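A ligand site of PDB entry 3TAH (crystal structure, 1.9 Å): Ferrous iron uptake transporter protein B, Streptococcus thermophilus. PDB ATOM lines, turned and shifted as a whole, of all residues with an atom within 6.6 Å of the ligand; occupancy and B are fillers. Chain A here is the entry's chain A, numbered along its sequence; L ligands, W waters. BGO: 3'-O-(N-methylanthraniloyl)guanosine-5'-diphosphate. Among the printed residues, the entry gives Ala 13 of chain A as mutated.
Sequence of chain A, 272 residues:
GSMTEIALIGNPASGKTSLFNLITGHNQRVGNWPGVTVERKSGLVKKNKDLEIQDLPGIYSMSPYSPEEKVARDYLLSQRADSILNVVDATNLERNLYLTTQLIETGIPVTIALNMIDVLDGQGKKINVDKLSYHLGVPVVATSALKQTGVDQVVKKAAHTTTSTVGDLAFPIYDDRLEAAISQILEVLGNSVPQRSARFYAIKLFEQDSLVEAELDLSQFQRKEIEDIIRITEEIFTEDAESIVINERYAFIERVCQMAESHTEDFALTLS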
ATOM      1  N   GLY A  10      24.579  20.973 -10.123  1.00  0.00           N
ATOM      2  CA  GLY A  10      25.637  20.008  -9.832  1.00  0.00           C
ATOM      3  C   GLY A  10      25.227  18.665 -10.408  1.00  0.00           C
ATOM      4  O   GLY A  10      24.145  18.534 -11.000  1.00  0.00           O
ATOM      5  N   ASN A  11      26.107  17.680 -10.230  1.00  0.00           N
ATOM      6  CA  ASN A  11      25.839  16.326 -10.657  1.00  0.00           C
ATOM      7  C   ASN A  11      24.672  15.731  -9.847  1.00  0.00           C
ATOM      8  O   ASN A  11      24.425  16.139  -8.710  1.00  0.00           O
ATOM      9  CB  ASN A  11      27.024  15.410 -10.367  1.00  0.00           C
ATOM     10  CG  ASN A  11      28.270  15.681 -11.204  1.00  0.00           C
ATOM     11  OD1 ASN A  11      29.278  15.016 -10.958  1.00  0.00           O
ATOM     12  ND2 ASN A  11      28.238  16.600 -12.166  1.00  0.00           N
ATOM     13  N   PRO A  12      23.982  14.750 -10.428  1.00  0.00           N
ATOM     14  CA  PRO A  12      23.089  13.897  -9.641  1.00  0.00           C
ATOM     15  C   PRO A  12      23.799  13.333  -8.432  1.00  0.00           C
ATOM     16  O   PRO A  12      24.986  12.974  -8.512  1.00  0.00           O
ATOM     17  CB  PRO A  12      22.739  12.762 -10.610  1.00  0.00           C
ATOM     18  CG  PRO A  12      22.815  13.412 -11.940  1.00  0.00           C
ATOM     19  CD  PRO A  12      23.978  14.339 -11.852  1.00  0.00           C
ATOM     20  N   ALA A  13      23.077  13.264  -7.318  1.00  0.00           N
ATOM     21  CA  ALA A  13      23.569  12.678  -6.071  1.00  0.00           C
ATOM     22  C   ALA A  13      24.748  13.448  -5.482  1.00  0.00           C
ATOM     23  O   ALA A  13      25.565  12.883  -4.758  1.00  0.00           O
ATOM     24  CB  ALA A  13      23.921  11.169  -6.261  1.00  0.00           C
ATOM     25  N   SER A  14      24.858  14.741  -5.780  1.00  0.00           N
ATOM     26  CA  SER A  14      25.900  15.578  -5.226  1.00  0.00           C
ATOM     27  C   SER A  14      25.448  16.236  -3.932  1.00  0.00           C
ATOM     28  O   SER A  14      26.258  16.827  -3.214  1.00  0.00           O
ATOM     29  CB  SER A  14      26.347  16.633  -6.233  1.00  0.00           C
ATOM     30  OG  SER A  14      25.303  17.529  -6.545  1.00  0.00           O
ATOM     31  N   GLY A  15      24.166  16.141  -3.634  1.00  0.00           N
ATOM     32  CA  GLY A  15      23.562  16.796  -2.474  1.00  0.00           C
ATOM     33  C   GLY A  15      22.859  18.104  -2.825  1.00  0.00           C
ATOM     34  O   GLY A  15      22.564  18.913  -1.943  1.00  0.00           O
ATOM     35  N   LYS A  16      22.578  18.314  -4.121  1.00  0.00           N
ATOM     36  CA  LYS A  16      21.974  19.559  -4.569  1.00  0.00           C
ATOM     37  C   LYS A  16      20.575  19.748  -3.972  1.00  0.00           C
ATOM     38  O   LYS A  16      20.267  20.823  -3.466  1.00  0.00           O
ATOM     39  CB  LYS A  16      21.957  19.652  -6.098  1.00  0.00           C
ATOM     40  CG  LYS A  16      21.216  20.883  -6.624  1.00  0.00           C
ATOM     41  CD  LYS A  16      21.396  21.065  -8.114  1.00  0.00           C
ATOM     42  CE  LYS A  16      20.701  19.983  -8.905  1.00  0.00           C
ATOM     43  NZ  LYS A  16      19.221  20.034  -8.759  1.00  0.00           N
ATOM     44  N   THR A  17      19.739  18.710  -4.019  1.00  0.00           N
ATOM     45  CA  THR A  17      18.394  18.786  -3.453  1.00  0.00           C
ATOM     46  C   THR A  17      18.448  19.024  -1.941  1.00  0.00           C
ATOM     47  O   THR A  17      17.691  19.849  -1.417  1.00  0.00           O
ATOM     48  CB  THR A  17      17.565  17.500  -3.694  1.00  0.00           C
ATOM     49  OG1 THR A  17      17.460  17.263  -5.097  1.00  0.00           O
ATOM     50  CG2 THR A  17      16.173  17.648  -3.109  1.00  0.00           C
ATOM     51  N   SER A  18      19.326  18.294  -1.267  1.00  0.00           N
ATOM     52  CA  SER A  18      19.503  18.447   0.178  1.00  0.00           C
ATOM     53  C   SER A  18      19.851  19.878   0.528  1.00  0.00           C
ATOM     54  O   SER A  18      19.286  20.423   1.474  1.00  0.00           O
ATOM     55  CB  SER A  18      20.569  17.494   0.722  1.00  0.00           C
ATOM     56  OG  SER A  18      20.186  16.139   0.557  1.00  0.00           O
ATOM     57  N   LEU A  19      20.792  20.476  -0.214  1.00  0.00           N
ATOM     58  CA  LEU A  19      21.155  21.886   0.023  1.00  0.00           C
ATOM     59  C   LEU A  19      20.024  22.831  -0.389  1.00  0.00           C
ATOM     60  O   LEU A  19      19.731  23.775   0.324  1.00  0.00           O
ATOM     61  CB  LEU A  19      22.441  22.288  -0.711  1.00  0.00           C
ATOM     62  CG  LEU A  19      23.715  21.628  -0.185  1.00  0.00           C
ATOM     63  CD1 LEU A  19      24.895  21.906  -1.119  1.00  0.00           C
ATOM     64  CD2 LEU A  19      24.052  22.096   1.214  1.00  0.00           C
ATOM     65  N   GLY A  58      19.962  18.135 -12.151  1.00  0.00           N
ATOM     66  CA  GLY A  58      21.256  17.526 -11.923  1.00  0.00           C
ATOM     67  C   GLY A  58      21.790  16.974 -13.238  1.00  0.00           C
ATOM     68  O   GLY A  58      21.112  16.186 -13.907  1.00  0.00           O
ATOM     69  N   VAL A  87      27.175  22.881  -6.801  1.00  0.00           N
ATOM     70  CA  VAL A  87      27.280  21.836  -5.752  1.00  0.00           C
ATOM     71  C   VAL A  87      28.170  20.715  -6.285  1.00  0.00           C
ATOM     72  O   VAL A  87      27.872  20.101  -7.321  1.00  0.00           O
ATOM     73  CB  VAL A  87      25.888  21.290  -5.348  1.00  0.00           C
ATOM     74  CG1 VAL A  87      26.009  20.235  -4.243  1.00  0.00           C
ATOM     75  CG2 VAL A  87      24.979  22.435  -4.904  1.00  0.00           C
ATOM     76  N   ASN A 115      30.512  20.004  -1.198  1.00  0.00           N
ATOM     77  CA  ASN A 115      29.559  19.285  -0.357  1.00  0.00           C
ATOM     78  C   ASN A 115      30.044  17.861  -0.016  1.00  0.00           C
ATOM     79  O   ASN A 115      31.020  17.390  -0.595  1.00  0.00           O
ATOM     80  CB  ASN A 115      28.166  19.315  -1.020  1.00  0.00           C
ATOM     81  CG  ASN A 115      27.026  18.945  -0.074  1.00  0.00           C
ATOM     82  OD1 ASN A 115      26.927  19.476   1.034  1.00  0.00           O
ATOM     83  ND2 ASN A 115      26.160  18.027  -0.516  1.00  0.00           N
ATOM     84  N   MET A 116      29.387  17.186   0.921  1.00  0.00           N
ATOM     85  CA  MET A 116      29.800  15.856   1.389  1.00  0.00           C
ATOM     86  C   MET A 116      31.125  15.905   2.142  1.00  0.00           C
ATOM     87  O   MET A 116      31.812  14.878   2.225  1.00  0.00           O
ATOM     88  CB  MET A 116      29.953  14.851   0.247  1.00  0.00           C
ATOM     89  CG  MET A 116      28.731  14.702  -0.607  1.00  0.00           C
ATOM     90  SD  MET A 116      27.613  13.496   0.128  1.00  0.00           S
ATOM     91  CE  MET A 116      26.272  13.635  -1.034  1.00  0.00           C
ATOM     92  N   ILE A 117      31.490  17.071   2.670  1.00  0.00           N
ATOM     93  CA  ILE A 117      32.781  17.249   3.325  1.00  0.00           C
ATOM     94  C   ILE A 117      32.919  16.347   4.573  1.00  0.00           C
ATOM     95  O   ILE A 117      34.029  15.924   4.927  1.00  0.00           O
ATOM     96  CB  ILE A 117      33.066  18.764   3.612  1.00  0.00           C
ATOM     97  CG1 ILE A 117      34.558  19.054   3.552  1.00  0.00           C
ATOM     98  CG2 ILE A 117      32.432  19.228   4.945  1.00  0.00           C
ATOM     99  CD1 ILE A 117      35.141  18.945   2.136  1.00  0.00           C
ATOM    100  N   ASP A 118      31.793  16.053   5.220  1.00  0.00           N
ATOM    101  CA  ASP A 118      31.798  15.159   6.393  1.00  0.00           C
ATOM    102  C   ASP A 118      32.126  13.698   6.043  1.00  0.00           C
ATOM    103  O   ASP A 118      32.651  12.977   6.889  1.00  0.00           O
ATOM    104  CB  ASP A 118      30.435  15.211   7.104  1.00  0.00           C
ATOM    105  CG  ASP A 118      29.302  14.766   6.213  1.00  0.00           C
ATOM    106  OD1 ASP A 118      29.010  15.467   5.227  1.00  0.00           O
ATOM    107  OD2 ASP A 118      28.678  13.707   6.473  1.00  0.00           O
ATOM    108  N   VAL A 119      31.791  13.279   4.832  1.00  0.00           N
ATOM    109  CA  VAL A 119      32.022  11.926   4.314  1.00  0.00           C
ATOM    110  C   VAL A 119      33.502  11.728   3.994  1.00  0.00           C
ATOM    111  O   VAL A 119      34.075  10.669   4.250  1.00  0.00           O
ATOM    112  CB  VAL A 119      31.214  11.663   3.010  1.00  0.00           C
ATOM    113  CG1 VAL A 119      31.422  10.231   2.499  1.00  0.00           C
ATOM    114  CG2 VAL A 119      29.741  11.927   3.232  1.00  0.00           C
ATOM    115  N   THR A 143      30.931  22.471   2.524  1.00  0.00           N
ATOM    116  CA  THR A 143      29.611  22.315   3.105  1.00  0.00           C
ATOM    117  C   THR A 143      29.299  20.852   3.424  1.00  0.00           C
ATOM    118  O   THR A 143      29.887  19.927   2.865  1.00  0.00           O
ATOM    119  CB  THR A 143      28.476  22.853   2.175  1.00  0.00           C
ATOM    120  OG1 THR A 143      28.395  22.055   0.991  1.00  0.00           O
ATOM    121  CG2 THR A 143      28.689  24.302   1.793  1.00  0.00           C
ATOM    122  N   SER A 144      28.341  20.689   4.336  1.00  0.00           N
ATOM    123  CA  SER A 144      27.718  19.398   4.613  1.00  0.00           C
ATOM    124  C   SER A 144      26.224  19.626   4.763  1.00  0.00           C
ATOM    125  O   SER A 144      25.793  20.304   5.694  1.00  0.00           O
ATOM    126  CB  SER A 144      28.272  18.751   5.888  1.00  0.00           C
ATOM    127  OG  SER A 144      27.638  17.505   6.116  1.00  0.00           O
ATOM    128  N   ALA A 145      25.444  19.085   3.822  1.00  0.00           N
ATOM    129  CA  ALA A 145      23.988  19.136   3.895  1.00  0.00           C
ATOM    130  C   ALA A 145      23.487  18.297   5.083  1.00  0.00           C
ATOM    131  O   ALA A 145      22.508  18.655   5.727  1.00  0.00           O
ATOM    132  CB  ALA A 145      23.355  18.679   2.572  1.00  0.00           C
ATOM    133  N   LEU A 146      24.183  17.194   5.392  1.00  0.00           N
ATOM    134  CA  LEU A 146      23.798  16.332   6.516  1.00  0.00           C
ATOM    135  C   LEU A 146      24.007  17.039   7.860  1.00  0.00           C
ATOM    136  O   LEU A 146      23.061  17.229   8.654  1.00  0.00           O
ATOM    137  CB  LEU A 146      24.568  15.006   6.481  1.00  0.00           C
ATOM    138  CG  LEU A 146      24.332  14.034   7.664  1.00  0.00           C
ATOM    139  CD1 LEU A 146      22.864  13.673   7.778  1.00  0.00           C
ATOM    140  CD2 LEU A 146      25.186  12.786   7.493  1.00  0.00           C
ATOM    141  N   LYS A 147      25.252  17.462   8.102  1.00  0.00           N
ATOM    142  CA  LYS A 147      25.625  18.136   9.346  1.00  0.00           C
ATOM    143  C   LYS A 147      25.134  19.583   9.411  1.00  0.00           C
ATOM    144  O   LYS A 147      25.205  20.197  10.471  1.00  0.00           O
ATOM    145  CB  LYS A 147      27.144  18.113   9.538  1.00  0.00           C
ATOM    146  CG  LYS A 147      27.789  16.724   9.466  1.00  0.00           C
ATOM    147  CD  LYS A 147      27.289  15.770  10.545  1.00  0.00           C
ATOM    148  CE  LYS A 147      27.751  14.340  10.287  1.00  0.00           C
ATOM    149  NZ  LYS A 147      27.038  13.369  11.183  1.00  0.00           N
HETATM  150  C'  BGO L   1      20.045   9.788   0.989  1.00  0.00           C
HETATM  151  N1  BGO L   1      26.805  14.733   3.591  1.00  0.00           N
HETATM  152  C2  BGO L   1      26.323  13.412   3.677  1.00  0.00           C
HETATM  153  N2  BGO L   1      26.897  12.555   4.513  1.00  0.00           N
HETATM  154  N3  BGO L   1      25.295  13.031   2.910  1.00  0.00           N
HETATM  155  C4  BGO L   1      24.719  13.921   2.070  1.00  0.00           C
HETATM  156  C5  BGO L   1      25.156  15.248   1.942  1.00  0.00           C
HETATM  157  C6  BGO L   1      26.231  15.672   2.729  1.00  0.00           C
HETATM  158  O6  BGO L   1      26.662  16.824   2.682  1.00  0.00           O
HETATM  159  N7  BGO L   1      24.373  15.828   1.036  1.00  0.00           N
HETATM  160  C8  BGO L   1      23.485  14.939   0.585  1.00  0.00           C
HETATM  161  N9  BGO L   1      23.706  13.784   1.238  1.00  0.00           N
HETATM  162  PA  BGO L   1      20.646  14.554  -2.888  1.00  0.00           P
HETATM  163  PB  BGO L   1      20.907  15.512  -5.626  1.00  0.00           P
HETATM  164  C1' BGO L   1      20.079   8.404   1.673  1.00  0.00           C
HETATM  165  O1' BGO L   1      19.017  10.449   0.946  1.00  0.00           O
HETATM  166  O1A BGO L   1      20.418  15.867  -2.280  1.00  0.00           O
HETATM  167  C1B BGO L   1      23.058  12.511   1.126  1.00  0.00           C
HETATM  168  O1B BGO L   1      22.097  16.179  -6.160  1.00  0.00           O
HETATM  169  C2' BGO L   1      19.006   7.954   2.459  1.00  0.00           C
HETATM  170  N2' BGO L   1      17.912   8.695   2.646  1.00  0.00           N
HETATM  171  O2' BGO L   1      20.937  12.437   2.115  1.00  0.00           O
HETATM  172  O2A BGO L   1      19.477  13.663  -3.182  1.00  0.00           O
HETATM  173  C2B BGO L   1      21.638  12.446   0.894  1.00  0.00           C
HETATM  174  O2B BGO L   1      19.818  16.391  -5.259  1.00  0.00           O
HETATM  175  C3' BGO L   1      19.097   6.708   3.051  1.00  0.00           C
HETATM  176  O3' BGO L   1      21.139  10.283   0.468  1.00  0.00           O
HETATM  177  O3A BGO L   1      21.442  14.724  -4.291  1.00  0.00           O
HETATM  178  C3B BGO L   1      20.985  11.598  -0.098  1.00  0.00           C
HETATM  179  O3B BGO L   1      20.471  14.344  -6.459  1.00  0.00           O
HETATM  180  C4' BGO L   1      20.224   5.916   2.889  1.00  0.00           C
HETATM  181  O4' BGO L   1      23.427  12.017  -0.218  1.00  0.00           O
HETATM  182  C4B BGO L   1      22.208  11.548  -1.012  1.00  0.00           C
HETATM  183  C5' BGO L   1      21.289   6.348   2.108  1.00  0.00           C
HETATM  184  O5' BGO L   1      21.683  13.747  -1.969  1.00  0.00           O
HETATM  185  C5B BGO L   1      22.117  12.412  -2.283  1.00  0.00           C
HETATM  186  C6' BGO L   1      21.218   7.605   1.506  1.00  0.00           C
HETATM  187  CM' BGO L   1      16.606   8.114   3.016  1.00  0.00           C
HETATM  188  O   HOH W   1      18.501  13.493   2.394  1.00  0.00           O
HETATM  189  O   HOH W   2      25.888   9.989   5.552  1.00  0.00           O
HETATM  190  O   HOH W   3      21.912  17.013  -8.533  1.00  0.00           O
HETATM  191  O   HOH W   4      17.259  13.950  -1.562  1.00  0.00           O
HETATM  192  O   HOH W   5      25.706  10.235   2.051  1.00  0.00           O
HETATM  193  O   HOH W   6      19.974  11.975  -5.622  1.00  0.00           O
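Water W3 bridges an oxygen (O1B) of the ligand (2.5 Å) and the backbone carbonyl oxygen (O) of Asn 11 (2.7 Å).
An oxygen (O1B) of the ligand sits close to the backbone carbonyl oxygen (O) of Asn 11 (3.5 Å).
Pro 12 touches the ligand.
Val 119 touches the ligand.
CA of Ser 144 touches O6 of the ligand, 3.4 Å away.
Leu 146 touches the ligand (CD2 to N2, 3.4 Å).
Hydrophobic or aromatic side chains that line the ligand: Met 116, Val 119, Ala 145 and Leu 146.
Within 4 Å of the ligand: Asn 11, Pro 12, Ala 13, Ser 14, Gly 15, Lys 16, Thr 17, Ser 18, Asn 115, Met 116, Asp 118, Val 119, Ser 144, Ala 145 and Leu 146.
The nearest printed residue that does not touch the ligand is Thr 143 (4.5 Å).
The side-chain amide oxygen (OD1) of Asn 115 sits at hydrogen-bond distance from the backbone NH (N) of Ala 145 (3.2 Å).
OD1 of Asp 118 sits at hydrogen-bond distance from OG of Ser 144 (2.6 Å).
The backbone carbonyl oxygen of Ser 14 sits at hydrogen-bond distance from the side-chain amide nitrogen of Asn 115.
OD1 of Asn 115 lies within hydrogen-bond range of OG1 of Thr 143 (3.0 Å).
O of Asn 11 sits at hydrogen-bond distance from OG of Ser 14, at 2.7 Å.
N of Met 116 is in hydrogen-bond range of O of Thr 143 (3.4 Å).
The backbone NH (N) of Lys 147 sits at hydrogen-bond distance from the side-chain hydroxyl (OG) of Ser 144, 3.1 Å away.
An oxygen (O2B) of the ligand lies within hydrogen-bond range of the backbone NH of Thr 17 (2.6 Å).
The side-chain hydroxyl (OG1) of Thr 17 lies within hydrogen-bond range of an oxygen (O2B) of the ligand (2.5 Å).
The backbone NH of Ala 145 sits at hydrogen-bond distance from an oxygen (O6) of the ligand, 2.8 Å away.
The side-chain carboxylate of Asp 118 lies within hydrogen-bond range of a nitrogen (N1) of the ligand (2.8 Å).
N of Ser 18 lies within hydrogen-bond range of O1A of the ligand, 2.8 Å away.
The side-chain hydroxyl (OG) of Ser 18 is in hydrogen-bond range of an oxygen (O1A) of the ligand, 2.9 Å away.
N of Ala 13 lies within hydrogen-bond range of O3B of the ligand, 2.9 Å away.
The backbone NH of Lys 16 sits at hydrogen-bond distance from an oxygen (O1B) of the ligand.
An oxygen (O6) of the ligand lies close to the side-chain amide oxygen (OD1) of Asn 115.
N of Ser 14 sits at hydrogen-bond distance from O1B of the ligand.
O3A of the ligand lies within hydrogen-bond range of N of Gly 15 (3.1 Å).
An oxygen (O6) of the ligand sits at hydrogen-bond distance from the backbone NH (N) of Met 116, at 3.3 Å.
The side-chain sulfur (SD) of Met 116 lies close to a nitrogen (N1) of the ligand (3.8 Å).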
